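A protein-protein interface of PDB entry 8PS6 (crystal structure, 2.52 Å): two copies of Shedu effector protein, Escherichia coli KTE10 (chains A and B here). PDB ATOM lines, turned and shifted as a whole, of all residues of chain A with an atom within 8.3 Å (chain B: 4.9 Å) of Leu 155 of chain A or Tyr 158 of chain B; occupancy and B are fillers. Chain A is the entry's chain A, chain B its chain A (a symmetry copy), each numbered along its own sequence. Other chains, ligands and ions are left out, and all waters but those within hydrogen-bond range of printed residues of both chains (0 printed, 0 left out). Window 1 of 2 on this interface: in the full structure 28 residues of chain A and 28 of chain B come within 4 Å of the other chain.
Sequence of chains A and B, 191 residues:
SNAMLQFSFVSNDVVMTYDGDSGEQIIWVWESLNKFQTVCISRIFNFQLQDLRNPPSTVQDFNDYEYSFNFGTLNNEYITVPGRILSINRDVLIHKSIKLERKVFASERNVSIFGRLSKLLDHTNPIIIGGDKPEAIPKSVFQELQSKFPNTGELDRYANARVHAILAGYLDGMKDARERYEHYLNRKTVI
OE1 of Glu 108 of chain A is in salt-bridge range of NH1 of Arg 109 of chain B (3.9 Å). OD1 of Asp 156 of chain B is in salt-bridge range of NE of Arg 109 of chain A (2.7 Å). The side-chain hydroxyl (OG1) of Thr 152 of chain A is in hydrogen-bond range of the guanidinium group (NH2) of Arg 109 of chain B (2.6 Å). The side-chain hydroxyl of Tyr 158 of chain B is in hydrogen-bond range of the side-chain carboxylate of Glu 154 of chain A. The side-chain carboxylate of Glu 154 of chain A is in salt-bridge range of the guanidinium group of Arg 162 of chain B (3.8 Å). The side-chain carboxylate of Asp 156 of chain A lies within salt-bridge range of the guanidinium group of Arg 109 of chain B (2.7 Å). The side-chain carboxylate of Glu 154 of chain B sits at hydrogen-bond distance from the side-chain hydroxyl of Tyr 158 of chain A, 2.7 Å away. The guanidinium group (NE) of Arg 162 of chain A is in salt-bridge range of the side-chain carboxylate (OE2) of Glu 154 of chain B (3.8 Å).
OG of Ser 107 of chain A is in hydrogen-bond range of O of Pro 150 of chain A (3.5 Å). The backbone NH (N) of Glu 154 of chain A lies close to the side-chain amide nitrogen (ND2) of Asn 151 of chain A, 3.4 Å away. The backbone carbonyl oxygen (O) of Asp 156 of chain A sits at hydrogen-bond distance from the side-chain amide nitrogen (ND2) of Asn 160 of chain A, at 3.0 Å. The backbone carbonyl oxygen (O) of Asp 156 of chain B is in hydrogen-bond range of the side-chain amide nitrogen (ND2) of Asn 160 of chain B, at 3.0 Å.
Glu 108 of chain A touches Ala 159 of chain B (O to CB, 3.6 Å). Arg 109 of chain A touches Ala 159 of chain B (CB to CB, 3.8 Å). Val 111 of chain A touches Ala 159 of chain B (CG2 to CB, 3.8 Å). Asn 160 of chain B touches Val 111 of chain A (ND2 to CG2, 3.2 Å). Pro 150 of chain A touches Arg 162 of chain B (CD to CG, 3.8 Å). Leu 155 of chain A touches Arg 109 of chain B. Tyr 158 of chain B touches Leu 155 of chain A. CD2 of Tyr 158 of chain A touches CD2 of Leu 155 of chain B (3.5 Å). Tyr 158 of chain B touches Tyr 158 of chain A. Ala 159 of chain A touches Arg 109 of chain B (CB to CB, 3.8 Å).
Of chain B, only Arg 109 (3.3 Å) and Tyr 158 (3.5 Å) come within 4 Å of Leu 155 of chain A. Of chain A, only Glu 154, Leu 155 and Tyr 158 come within 4 Å of Tyr 158 of chain B. Printed residues of chain B within 4 Å of Glu 108 of chain A: Arg 109 and Ala 159. Printed residues of chain A within 4 Å of Leu 155 of chain B: Arg 109 and Tyr 158. Ala 161 of chain B touches none of the printed residues of chain A. The nearest residue of chain A that does not touch Tyr 158 of chain B is Pro 150 of chain A (4.8 Å). The nearest printed residue of chain B that does not touch Tyr 158 of chain A is Arg 109 of chain B (6.9 Å).
Of the 11 printed residues of chain B, 8 touch a printed residue of chain A. Hydrophobic or aromatic side chains of chain B that line the printed part of chain A: Leu 155, Tyr 158 and Ala 159. Printed residues of chain A that touch a printed residue of chain B: Glu 108, Arg 109, Val 111, Pro 150, Thr 152, Glu 154, Leu 155, Asp 156, Tyr 158, Ala 159 and Arg 162. Hydrophobic or aromatic side chains of chain A within 4 Å of the printed part of chain B: Val 111, Pro 150, Leu 155, Tyr 158 and Ala 159.
Arg 109 of chain A touches Leu 155 of chain B, and with the chains exchanged Leu 155 of chain A touches Arg 109 of chain B. Arg 109 of chain A touches Asp 156 of chain B, and with the chains exchanged Asp 156 of chain A touches Arg 109 of chain B. Glu 154 of chain A touches Arg 162 of chain B, and with the chains exchanged Arg 162 of chain A touches Glu 154 of chain B. Leu 155 of chain A touches Tyr 158 of chain B, and with the chains exchanged Tyr 158 of chain A touches Leu 155 of chain B. Positions printed for both chains: 109, 153, 154, 155, 156, 157, 158, 159, 160, 161 and 162.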
ATOM      1  N   SER A 107     -18.936 -13.238 -17.673  1.00  0.00           N
ATOM      2  CA  SER A 107     -19.618 -13.143 -16.393  1.00  0.00           C
ATOM      3  C   SER A 107     -20.439 -11.859 -16.361  1.00  0.00           C
ATOM      4  O   SER A 107     -20.380 -11.037 -17.277  1.00  0.00           O
ATOM      5  CB  SER A 107     -18.613 -13.183 -15.237  1.00  0.00           C
ATOM      6  OG  SER A 107     -19.275 -13.178 -13.987  1.00  0.00           O
ATOM      7  N   GLU A 108     -21.215 -11.696 -15.292  1.00  0.00           N
ATOM      8  CA  GLU A 108     -22.069 -10.522 -15.162  1.00  0.00           C
ATOM      9  C   GLU A 108     -21.247  -9.239 -15.244  1.00  0.00           C
ATOM     10  O   GLU A 108     -20.082  -9.194 -14.841  1.00  0.00           O
ATOM     11  CB  GLU A 108     -22.846 -10.576 -13.848  1.00  0.00           C
ATOM     12  CG  GLU A 108     -24.097 -11.434 -13.912  1.00  0.00           C
ATOM     13  CD  GLU A 108     -25.191 -10.796 -14.746  1.00  0.00           C
ATOM     14  OE1 GLU A 108     -25.497  -9.605 -14.516  1.00  0.00           O
ATOM     15  OE2 GLU A 108     -25.745 -11.483 -15.632  1.00  0.00           O
ATOM     16  N   ARG A 109     -21.875  -8.190 -15.786  1.00  0.00           N
ATOM     17  CA  ARG A 109     -21.226  -6.916 -16.105  1.00  0.00           C
ATOM     18  C   ARG A 109     -20.175  -7.062 -17.206  1.00  0.00           C
ATOM     19  O   ARG A 109     -19.183  -6.328 -17.228  1.00  0.00           O
ATOM     20  CB  ARG A 109     -20.609  -6.255 -14.865  1.00  0.00           C
ATOM     21  CG  ARG A 109     -21.618  -5.869 -13.799  1.00  0.00           C
ATOM     22  CD  ARG A 109     -22.710  -4.989 -14.372  1.00  0.00           C
ATOM     23  NE  ARG A 109     -22.222  -3.661 -14.720  1.00  0.00           N
ATOM     24  CZ  ARG A 109     -22.696  -2.533 -14.209  1.00  0.00           C
ATOM     25  NH1 ARG A 109     -23.694  -2.534 -13.341  1.00  0.00           N
ATOM     26  NH2 ARG A 109     -22.163  -1.375 -14.586  1.00  0.00           N
ATOM     27  N   ASN A 110     -20.386  -8.014 -18.122  1.00  0.00           N
ATOM     28  CA  ASN A 110     -19.569  -8.150 -19.331  1.00  0.00           C
ATOM     29  C   ASN A 110     -18.100  -8.415 -19.004  1.00  0.00           C
ATOM     30  O   ASN A 110     -17.196  -7.850 -19.622  1.00  0.00           O
ATOM     31  CB  ASN A 110     -19.710  -6.916 -20.226  1.00  0.00           C
ATOM     32  CG  ASN A 110     -21.154  -6.596 -20.553  1.00  0.00           C
ATOM     33  OD1 ASN A 110     -21.884  -7.434 -21.083  1.00  0.00           O
ATOM     34  ND2 ASN A 110     -21.577  -5.378 -20.231  1.00  0.00           N
ATOM     35  N   VAL A 111     -17.855  -9.283 -18.028  1.00  0.00           N
ATOM     36  CA  VAL A 111     -16.496  -9.639 -17.634  1.00  0.00           C
ATOM     37  C   VAL A 111     -16.013 -10.781 -18.519  1.00  0.00           C
ATOM     38  O   VAL A 111     -16.598 -11.870 -18.518  1.00  0.00           O
ATOM     39  CB  VAL A 111     -16.428 -10.029 -16.151  1.00  0.00           C
ATOM     40  CG1 VAL A 111     -15.020 -10.493 -15.798  1.00  0.00           C
ATOM     41  CG2 VAL A 111     -16.844  -8.859 -15.277  1.00  0.00           C
ATOM     42  N   LYS A 148     -19.143 -19.746  -9.005  1.00  0.00           N
ATOM     43  CA  LYS A 148     -18.595 -18.790  -8.051  1.00  0.00           C
ATOM     44  C   LYS A 148     -18.600 -17.369  -8.602  1.00  0.00           C
ATOM     45  O   LYS A 148     -18.681 -16.411  -7.824  1.00  0.00           O
ATOM     46  CB  LYS A 148     -17.176 -19.198  -7.651  1.00  0.00           C
ATOM     47  CG  LYS A 148     -17.103 -20.501  -6.872  1.00  0.00           C
ATOM     48  CD  LYS A 148     -15.665 -20.936  -6.648  1.00  0.00           C
ATOM     49  CE  LYS A 148     -15.600 -22.166  -5.757  1.00  0.00           C
ATOM     50  NZ  LYS A 148     -14.203 -22.635  -5.548  1.00  0.00           N
ATOM     51  N   PHE A 149     -18.518 -17.217  -9.923  1.00  0.00           N
ATOM     52  CA  PHE A 149     -18.537 -15.901 -10.539  1.00  0.00           C
ATOM     53  C   PHE A 149     -19.798 -15.141 -10.129  1.00  0.00           C
ATOM     54  O   PHE A 149     -20.854 -15.745  -9.912  1.00  0.00           O
ATOM     55  CB  PHE A 149     -18.476 -16.022 -12.062  1.00  0.00           C
ATOM     56  CG  PHE A 149     -17.161 -16.537 -12.583  1.00  0.00           C
ATOM     57  CD1 PHE A 149     -15.995 -16.361 -11.859  1.00  0.00           C
ATOM     58  CD2 PHE A 149     -17.094 -17.194 -13.801  1.00  0.00           C
ATOM     59  CE1 PHE A 149     -14.787 -16.832 -12.338  1.00  0.00           C
ATOM     60  CE2 PHE A 149     -15.887 -17.667 -14.287  1.00  0.00           C
ATOM     61  CZ  PHE A 149     -14.733 -17.486 -13.553  1.00  0.00           C
ATOM     62  N   PRO A 150     -19.719 -13.815 -10.014  1.00  0.00           N
ATOM     63  CA  PRO A 150     -20.876 -13.048  -9.533  1.00  0.00           C
ATOM     64  C   PRO A 150     -22.045 -13.120 -10.508  1.00  0.00           C
ATOM     65  O   PRO A 150     -21.883 -12.943 -11.719  1.00  0.00           O
ATOM     66  CB  PRO A 150     -20.327 -11.622  -9.407  1.00  0.00           C
ATOM     67  CG  PRO A 150     -19.173 -11.576 -10.355  1.00  0.00           C
ATOM     68  CD  PRO A 150     -18.565 -12.949 -10.312  1.00  0.00           C
ATOM     69  N   ASN A 151     -23.228 -13.387  -9.963  1.00  0.00           N
ATOM     70  CA  ASN A 151     -24.467 -13.452 -10.719  1.00  0.00           C
ATOM     71  C   ASN A 151     -25.243 -12.144 -10.550  1.00  0.00           C
ATOM     72  O   ASN A 151     -24.752 -11.173  -9.967  1.00  0.00           O
ATOM     73  CB  ASN A 151     -25.281 -14.669 -10.273  1.00  0.00           C
ATOM     74  CG  ASN A 151     -25.407 -14.767  -8.766  1.00  0.00           C
ATOM     75  OD1 ASN A 151     -24.501 -15.250  -8.085  1.00  0.00           O
ATOM     76  ND2 ASN A 151     -26.535 -14.311  -8.236  1.00  0.00           N
ATOM     77  N   THR A 152     -26.473 -12.111 -11.073  1.00  0.00           N
ATOM     78  CA  THR A 152     -27.280 -10.898 -10.976  1.00  0.00           C
ATOM     79  C   THR A 152     -27.656 -10.595  -9.531  1.00  0.00           C
ATOM     80  O   THR A 152     -27.674  -9.429  -9.121  1.00  0.00           O
ATOM     81  CB  THR A 152     -28.542 -11.023 -11.830  1.00  0.00           C
ATOM     82  OG1 THR A 152     -29.210  -9.757 -11.891  1.00  0.00           O
ATOM     83  CG2 THR A 152     -29.484 -12.064 -11.252  1.00  0.00           C
ATOM     84  N   GLY A 153     -27.960 -11.630  -8.747  1.00  0.00           N
ATOM     85  CA  GLY A 153     -28.368 -11.406  -7.370  1.00  0.00           C
ATOM     86  C   GLY A 153     -27.251 -10.852  -6.507  1.00  0.00           C
ATOM     87  O   GLY A 153     -27.485 -10.000  -5.646  1.00  0.00           O
ATOM     88  N   GLU A 154     -26.021 -11.325  -6.725  1.00  0.00           N
ATOM     89  CA  GLU A 154     -24.894 -10.825  -5.944  1.00  0.00           C
ATOM     90  C   GLU A 154     -24.631  -9.354  -6.241  1.00  0.00           C
ATOM     91  O   GLU A 154     -24.361  -8.568  -5.327  1.00  0.00           O
ATOM     92  CB  GLU A 154     -23.644 -11.661  -6.220  1.00  0.00           C
ATOM     93  CG  GLU A 154     -22.439 -11.215  -5.414  1.00  0.00           C
ATOM     94  CD  GLU A 154     -21.163 -11.921  -5.815  1.00  0.00           C
ATOM     95  OE1 GLU A 154     -21.230 -13.096  -6.237  1.00  0.00           O
ATOM     96  OE2 GLU A 154     -20.089 -11.296  -5.711  1.00  0.00           O
ATOM     97  N   LEU A 155     -24.704  -8.964  -7.516  1.00  0.00           N
ATOM     98  CA  LEU A 155     -24.536  -7.559  -7.868  1.00  0.00           C
ATOM     99  C   LEU A 155     -25.703  -6.715  -7.375  1.00  0.00           C
ATOM    100  O   LEU A 155     -25.515  -5.543  -7.028  1.00  0.00           O
ATOM    101  CB  LEU A 155     -24.372  -7.414  -9.379  1.00  0.00           C
ATOM    102  CG  LEU A 155     -23.091  -8.019  -9.951  1.00  0.00           C
ATOM    103  CD1 LEU A 155     -23.162  -8.038 -11.457  1.00  0.00           C
ATOM    104  CD2 LEU A 155     -21.882  -7.232  -9.486  1.00  0.00           C
ATOM    105  N   ASP A 156     -26.909  -7.286  -7.337  1.00  0.00           N
ATOM    106  CA  ASP A 156     -28.048  -6.551  -6.799  1.00  0.00           C
ATOM    107  C   ASP A 156     -27.905  -6.342  -5.298  1.00  0.00           C
ATOM    108  O   ASP A 156     -28.219  -5.261  -4.784  1.00  0.00           O
ATOM    109  CB  ASP A 156     -29.348  -7.286  -7.124  1.00  0.00           C
ATOM    110  CG  ASP A 156     -29.830  -7.024  -8.538  1.00  0.00           C
ATOM    111  OD1 ASP A 156     -29.285  -6.118  -9.202  1.00  0.00           O
ATOM    112  OD2 ASP A 156     -30.758  -7.729  -8.986  1.00  0.00           O
ATOM    113  N   ARG A 157     -27.427  -7.359  -4.578  1.00  0.00           N
ATOM    114  CA  ARG A 157     -27.227  -7.216  -3.141  1.00  0.00           C
ATOM    115  C   ARG A 157     -26.079  -6.267  -2.834  1.00  0.00           C
ATOM    116  O   ARG A 157     -26.152  -5.490  -1.874  1.00  0.00           O
ATOM    117  CB  ARG A 157     -26.973  -8.581  -2.503  1.00  0.00           C
ATOM    118  CG  ARG A 157     -28.216  -9.434  -2.337  1.00  0.00           C
ATOM    119  CD  ARG A 157     -27.891 -10.736  -1.623  1.00  0.00           C
ATOM    120  NE  ARG A 157     -26.937 -11.543  -2.374  1.00  0.00           N
ATOM    121  CZ  ARG A 157     -27.272 -12.422  -3.309  1.00  0.00           C
ATOM    122  NH1 ARG A 157     -28.537 -12.636  -3.636  1.00  0.00           N
ATOM    123  NH2 ARG A 157     -26.315 -13.103  -3.931  1.00  0.00           N
ATOM    124  N   TYR A 158     -25.006  -6.321  -3.628  1.00  0.00           N
ATOM    125  CA  TYR A 158     -23.889  -5.404  -3.425  1.00  0.00           C
ATOM    126  C   TYR A 158     -24.343  -3.955  -3.558  1.00  0.00           C
ATOM    127  O   TYR A 158     -24.045  -3.117  -2.697  1.00  0.00           O
ATOM    128  CB  TYR A 158     -22.767  -5.712  -4.419  1.00  0.00           C
ATOM    129  CG  TYR A 158     -21.647  -4.696  -4.395  1.00  0.00           C
ATOM    130  CD1 TYR A 158     -20.630  -4.776  -3.452  1.00  0.00           C
ATOM    131  CD2 TYR A 158     -21.610  -3.651  -5.310  1.00  0.00           C
ATOM    132  CE1 TYR A 158     -19.608  -3.846  -3.422  1.00  0.00           C
ATOM    133  CE2 TYR A 158     -20.592  -2.714  -5.289  1.00  0.00           C
ATOM    134  CZ  TYR A 158     -19.593  -2.816  -4.344  1.00  0.00           C
ATOM    135  OH  TYR A 158     -18.577  -1.885  -4.320  1.00  0.00           O
ATOM    136  N   ALA A 159     -25.094  -3.666  -4.620  1.00  0.00           N
ATOM    137  CA  ALA A 159     -25.562  -2.283  -4.854  1.00  0.00           C
ATOM    138  C   ALA A 159     -26.496  -1.856  -3.719  1.00  0.00           C
ATOM    139  O   ALA A 159     -26.333  -0.734  -3.217  1.00  0.00           O
ATOM    140  CB  ALA A 159     -26.230  -2.183  -6.198  1.00  0.00           C
ATOM    141  N   ASN A 160     -27.433  -2.724  -3.337  1.00  0.00           N
ATOM    142  CA  ASN A 160     -28.406  -2.380  -2.269  1.00  0.00           C
ATOM    143  C   ASN A 160     -27.669  -2.166  -0.945  1.00  0.00           C
ATOM    144  O   ASN A 160     -27.998  -1.201  -0.243  1.00  0.00           O
ATOM    145  CB  ASN A 160     -29.504  -3.437  -2.137  1.00  0.00           C
ATOM    146  CG  ASN A 160     -30.694  -3.162  -3.030  1.00  0.00           C
ATOM    147  OD1 ASN A 160     -31.724  -2.680  -2.567  1.00  0.00           O
ATOM    148  ND2 ASN A 160     -30.560  -3.460  -4.312  1.00  0.00           N
ATOM    149  N   ALA A 161     -26.705  -3.030  -0.631  1.00  0.00           N
ATOM    150  CA  ALA A 161     -25.943  -2.907   0.631  1.00  0.00           C
ATOM    151  C   ALA A 161     -25.146  -1.604   0.625  1.00  0.00           C
ATOM    152  O   ALA A 161     -25.091  -0.945   1.673  1.00  0.00           O
ATOM    153  CB  ALA A 161     -25.034  -4.095   0.800  1.00  0.00           C
ATOM    154  N   ARG A 162     -24.542  -1.269  -0.514  1.00  0.00           N
ATOM    155  CA  ARG A 162     -23.726  -0.035  -0.616  1.00  0.00           C
ATOM    156  C   ARG A 162     -24.635   1.176  -0.386  1.00  0.00           C
ATOM    157  O   ARG A 162     -24.248   2.056   0.394  1.00  0.00           O
ATOM    158  CB  ARG A 162     -23.042   0.007  -1.983  1.00  0.00           C
ATOM    159  CG  ARG A 162     -22.019   1.120  -2.147  1.00  0.00           C
ATOM    160  CD  ARG A 162     -20.626   0.674  -1.752  1.00  0.00           C
ATOM    161  NE  ARG A 162     -19.818   1.792  -1.290  1.00  0.00           N
ATOM    162  CZ  ARG A 162     -19.764   2.213  -0.032  1.00  0.00           C
ATOM    163  NH1 ARG A 162     -20.473   1.606   0.903  1.00  0.00           N
ATOM    164  NH2 ARG A 162     -18.998   3.240   0.288  1.00  0.00           N
ATOM    165  N   ARG B 109     -28.345  -0.769 -10.600  1.00  0.00           N
ATOM    166  CA  ARG B 109     -29.013  -2.041 -10.310  1.00  0.00           C
ATOM    167  C   ARG B 109     -30.409  -1.839  -9.718  1.00  0.00           C
ATOM    168  O   ARG B 109     -30.878  -2.657  -8.922  1.00  0.00           O
ATOM    169  CB  ARG B 109     -28.171  -2.938  -9.391  1.00  0.00           C
ATOM    170  CG  ARG B 109     -26.848  -3.375  -9.991  1.00  0.00           C
ATOM    171  CD  ARG B 109     -27.051  -4.045 -11.335  1.00  0.00           C
ATOM    172  NE  ARG B 109     -27.689  -5.349 -11.210  1.00  0.00           N
ATOM    173  CZ  ARG B 109     -27.153  -6.487 -11.629  1.00  0.00           C
ATOM    174  NH1 ARG B 109     -25.977  -6.515 -12.233  1.00  0.00           N
ATOM    175  NH2 ARG B 109     -27.819  -7.623 -11.447  1.00  0.00           N
ATOM    176  N   GLY B 153     -19.222   2.178 -13.143  1.00  0.00           N
ATOM    177  CA  GLY B 153     -17.822   1.794 -13.055  1.00  0.00           C
ATOM    178  C   GLY B 153     -17.507   1.009 -11.796  1.00  0.00           C
ATOM    179  O   GLY B 153     -16.711   0.065 -11.827  1.00  0.00           O
ATOM    180  N   GLU B 154     -18.124   1.382 -10.672  1.00  0.00           N
ATOM    181  CA  GLU B 154     -17.883   0.661  -9.427  1.00  0.00           C
ATOM    182  C   GLU B 154     -18.402  -0.769  -9.512  1.00  0.00           C
ATOM    183  O   GLU B 154     -17.742  -1.705  -9.049  1.00  0.00           O
ATOM    184  CB  GLU B 154     -18.524   1.398  -8.253  1.00  0.00           C
ATOM    185  CG  GLU B 154     -18.283   0.718  -6.918  1.00  0.00           C
ATOM    186  CD  GLU B 154     -19.063   1.344  -5.783  1.00  0.00           C
ATOM    187  OE1 GLU B 154     -19.308   2.569  -5.823  1.00  0.00           O
ATOM    188  OE2 GLU B 154     -19.436   0.605  -4.851  1.00  0.00           O
ATOM    189  N   LEU B 155     -19.587  -0.955 -10.098  1.00  0.00           N
ATOM    190  CA  LEU B 155     -20.116  -2.302 -10.280  1.00  0.00           C
ATOM    191  C   LEU B 155     -19.307  -3.088 -11.301  1.00  0.00           C
ATOM    192  O   LEU B 155     -19.176  -4.312 -11.177  1.00  0.00           O
ATOM    193  CB  LEU B 155     -21.583  -2.236 -10.698  1.00  0.00           C
ATOM    194  CG  LEU B 155     -22.533  -1.684  -9.635  1.00  0.00           C
ATOM    195  CD1 LEU B 155     -23.890  -1.434 -10.242  1.00  0.00           C
ATOM    196  CD2 LEU B 155     -22.641  -2.650  -8.472  1.00  0.00           C
ATOM    197  N   ASP B 156     -18.759  -2.411 -12.313  1.00  0.00           N
ATOM    198  CA  ASP B 156     -17.907  -3.099 -13.276  1.00  0.00           C
ATOM    199  C   ASP B 156     -16.601  -3.543 -12.632  1.00  0.00           C
ATOM    200  O   ASP B 156     -16.117  -4.651 -12.896  1.00  0.00           O
ATOM    201  CB  ASP B 156     -17.640  -2.197 -14.480  1.00  0.00           C
ATOM    202  CG  ASP B 156     -18.785  -2.195 -15.474  1.00  0.00           C
ATOM    203  OD1 ASP B 156     -19.694  -3.043 -15.348  1.00  0.00           O
ATOM    204  OD2 ASP B 156     -18.776  -1.342 -16.386  1.00  0.00           O
ATOM    205  N   ARG B 157     -16.017  -2.697 -11.781  1.00  0.00           N
ATOM    206  CA  ARG B 157     -14.783  -3.072 -11.098  1.00  0.00           C
ATOM    207  C   ARG B 157     -15.030  -4.167 -10.071  1.00  0.00           C
ATOM    208  O   ARG B 157     -14.197  -5.067  -9.907  1.00  0.00           O
ATOM    209  CB  ARG B 157     -14.155  -1.850 -10.431  1.00  0.00           C
ATOM    210  CG  ARG B 157     -13.446  -0.911 -11.388  1.00  0.00           C
ATOM    211  CD  ARG B 157     -12.781   0.231 -10.636  1.00  0.00           C
ATOM    212  NE  ARG B 157     -13.751   1.040  -9.910  1.00  0.00           N
ATOM    213  CZ  ARG B 157     -14.397   2.079 -10.425  1.00  0.00           C
ATOM    214  NH1 ARG B 157     -14.199   2.465 -11.676  1.00  0.00           N
ATOM    215  NH2 ARG B 157     -15.262   2.745  -9.668  1.00  0.00           N
ATOM    216  N   TYR B 158     -16.161  -4.104  -9.364  1.00  0.00           N
ATOM    217  CA  TYR B 158     -16.490  -5.148  -8.398  1.00  0.00           C
ATOM    218  C   TYR B 158     -16.586  -6.508  -9.080  1.00  0.00           C
ATOM    219  O   TYR B 158     -15.990  -7.491  -8.619  1.00  0.00           O
ATOM    220  CB  TYR B 158     -17.797  -4.810  -7.679  1.00  0.00           C
ATOM    221  CG  TYR B 158     -18.300  -5.926  -6.791  1.00  0.00           C
ATOM    222  CD1 TYR B 158     -17.808  -6.090  -5.502  1.00  0.00           C
ATOM    223  CD2 TYR B 158     -19.261  -6.821  -7.244  1.00  0.00           C
ATOM    224  CE1 TYR B 158     -18.261  -7.113  -4.689  1.00  0.00           C
ATOM    225  CE2 TYR B 158     -19.721  -7.849  -6.439  1.00  0.00           C
ATOM    226  CZ  TYR B 158     -19.218  -7.990  -5.163  1.00  0.00           C
ATOM    227  OH  TYR B 158     -19.674  -9.012  -4.358  1.00  0.00           O
ATOM    228  N   ALA B 159     -17.309  -6.559 -10.199  1.00  0.00           N
ATOM    229  CA  ALA B 159     -17.485  -7.837 -10.920  1.00  0.00           C
ATOM    230  C   ALA B 159     -16.131  -8.332 -11.432  1.00  0.00           C
ATOM    231  O   ALA B 159     -15.844  -9.527 -11.267  1.00  0.00           O
ATOM    232  CB  ALA B 159     -18.480  -7.668 -12.036  1.00  0.00           C
ATOM    233  N   ASN B 160     -15.338  -7.442 -12.027  1.00  0.00           N
ATOM    234  CA  ASN B 160     -14.022  -7.841 -12.587  1.00  0.00           C
ATOM    235  C   ASN B 160     -13.104  -8.323 -11.462  1.00  0.00           C
ATOM    236  O   ASN B 160     -12.431  -9.343 -11.656  1.00  0.00           O
ATOM    237  CB  ASN B 160     -13.379  -6.710 -13.393  1.00  0.00           C
ATOM    238  CG  ASN B 160     -13.779  -6.728 -14.852  1.00  0.00           C
ATOM    239  OD1 ASN B 160     -13.012  -7.168 -15.705  1.00  0.00           O
ATOM    240  ND2 ASN B 160     -14.979  -6.257 -15.149  1.00  0.00           N
ATOM    241  N   ALA B 161     -13.092  -7.617 -10.333  1.00  0.00           N
ATOM    242  CA  ALA B 161     -12.231  -8.002  -9.194  1.00  0.00           C
ATOM    243  C   ALA B 161     -12.668  -9.363  -8.656  1.00  0.00           C
ATOM    244  O   ALA B 161     -11.792 -10.172  -8.325  1.00  0.00           O
ATOM    245  CB  ALA B 161     -12.300  -6.950  -8.119  1.00  0.00           C
ATOM    246  N   ARG B 162     -13.979  -9.584  -8.562  1.00  0.00           N
ATOM    247  CA  ARG B 162     -14.505 -10.865  -8.032  1.00  0.00           C
ATOM    248  C   ARG B 162     -14.071 -11.999  -8.966  1.00  0.00           C
ATOM    249  O   ARG B 162     -13.589 -13.019  -8.459  1.00  0.00           O
ATOM    250  CB  ARG B 162     -16.027 -10.771  -7.903  1.00  0.00           C
ATOM    251  CG  ARG B 162     -16.676 -11.945  -7.187  1.00  0.00           C
ATOM    252  CD  ARG B 162     -16.794 -11.704  -5.695  1.00  0.00           C
ATOM    253  NE  ARG B 162     -16.786 -12.955  -4.951  1.00  0.00           N
ATOM    254  CZ  ARG B 162     -15.692 -13.562  -4.509  1.00  0.00           C
ATOM    255  NH1 ARG B 162     -14.502 -13.032  -4.734  1.00  0.00           N
ATOM    256  NH2 ARG B 162     -15.791 -14.697  -3.841  1.00  0.00           N
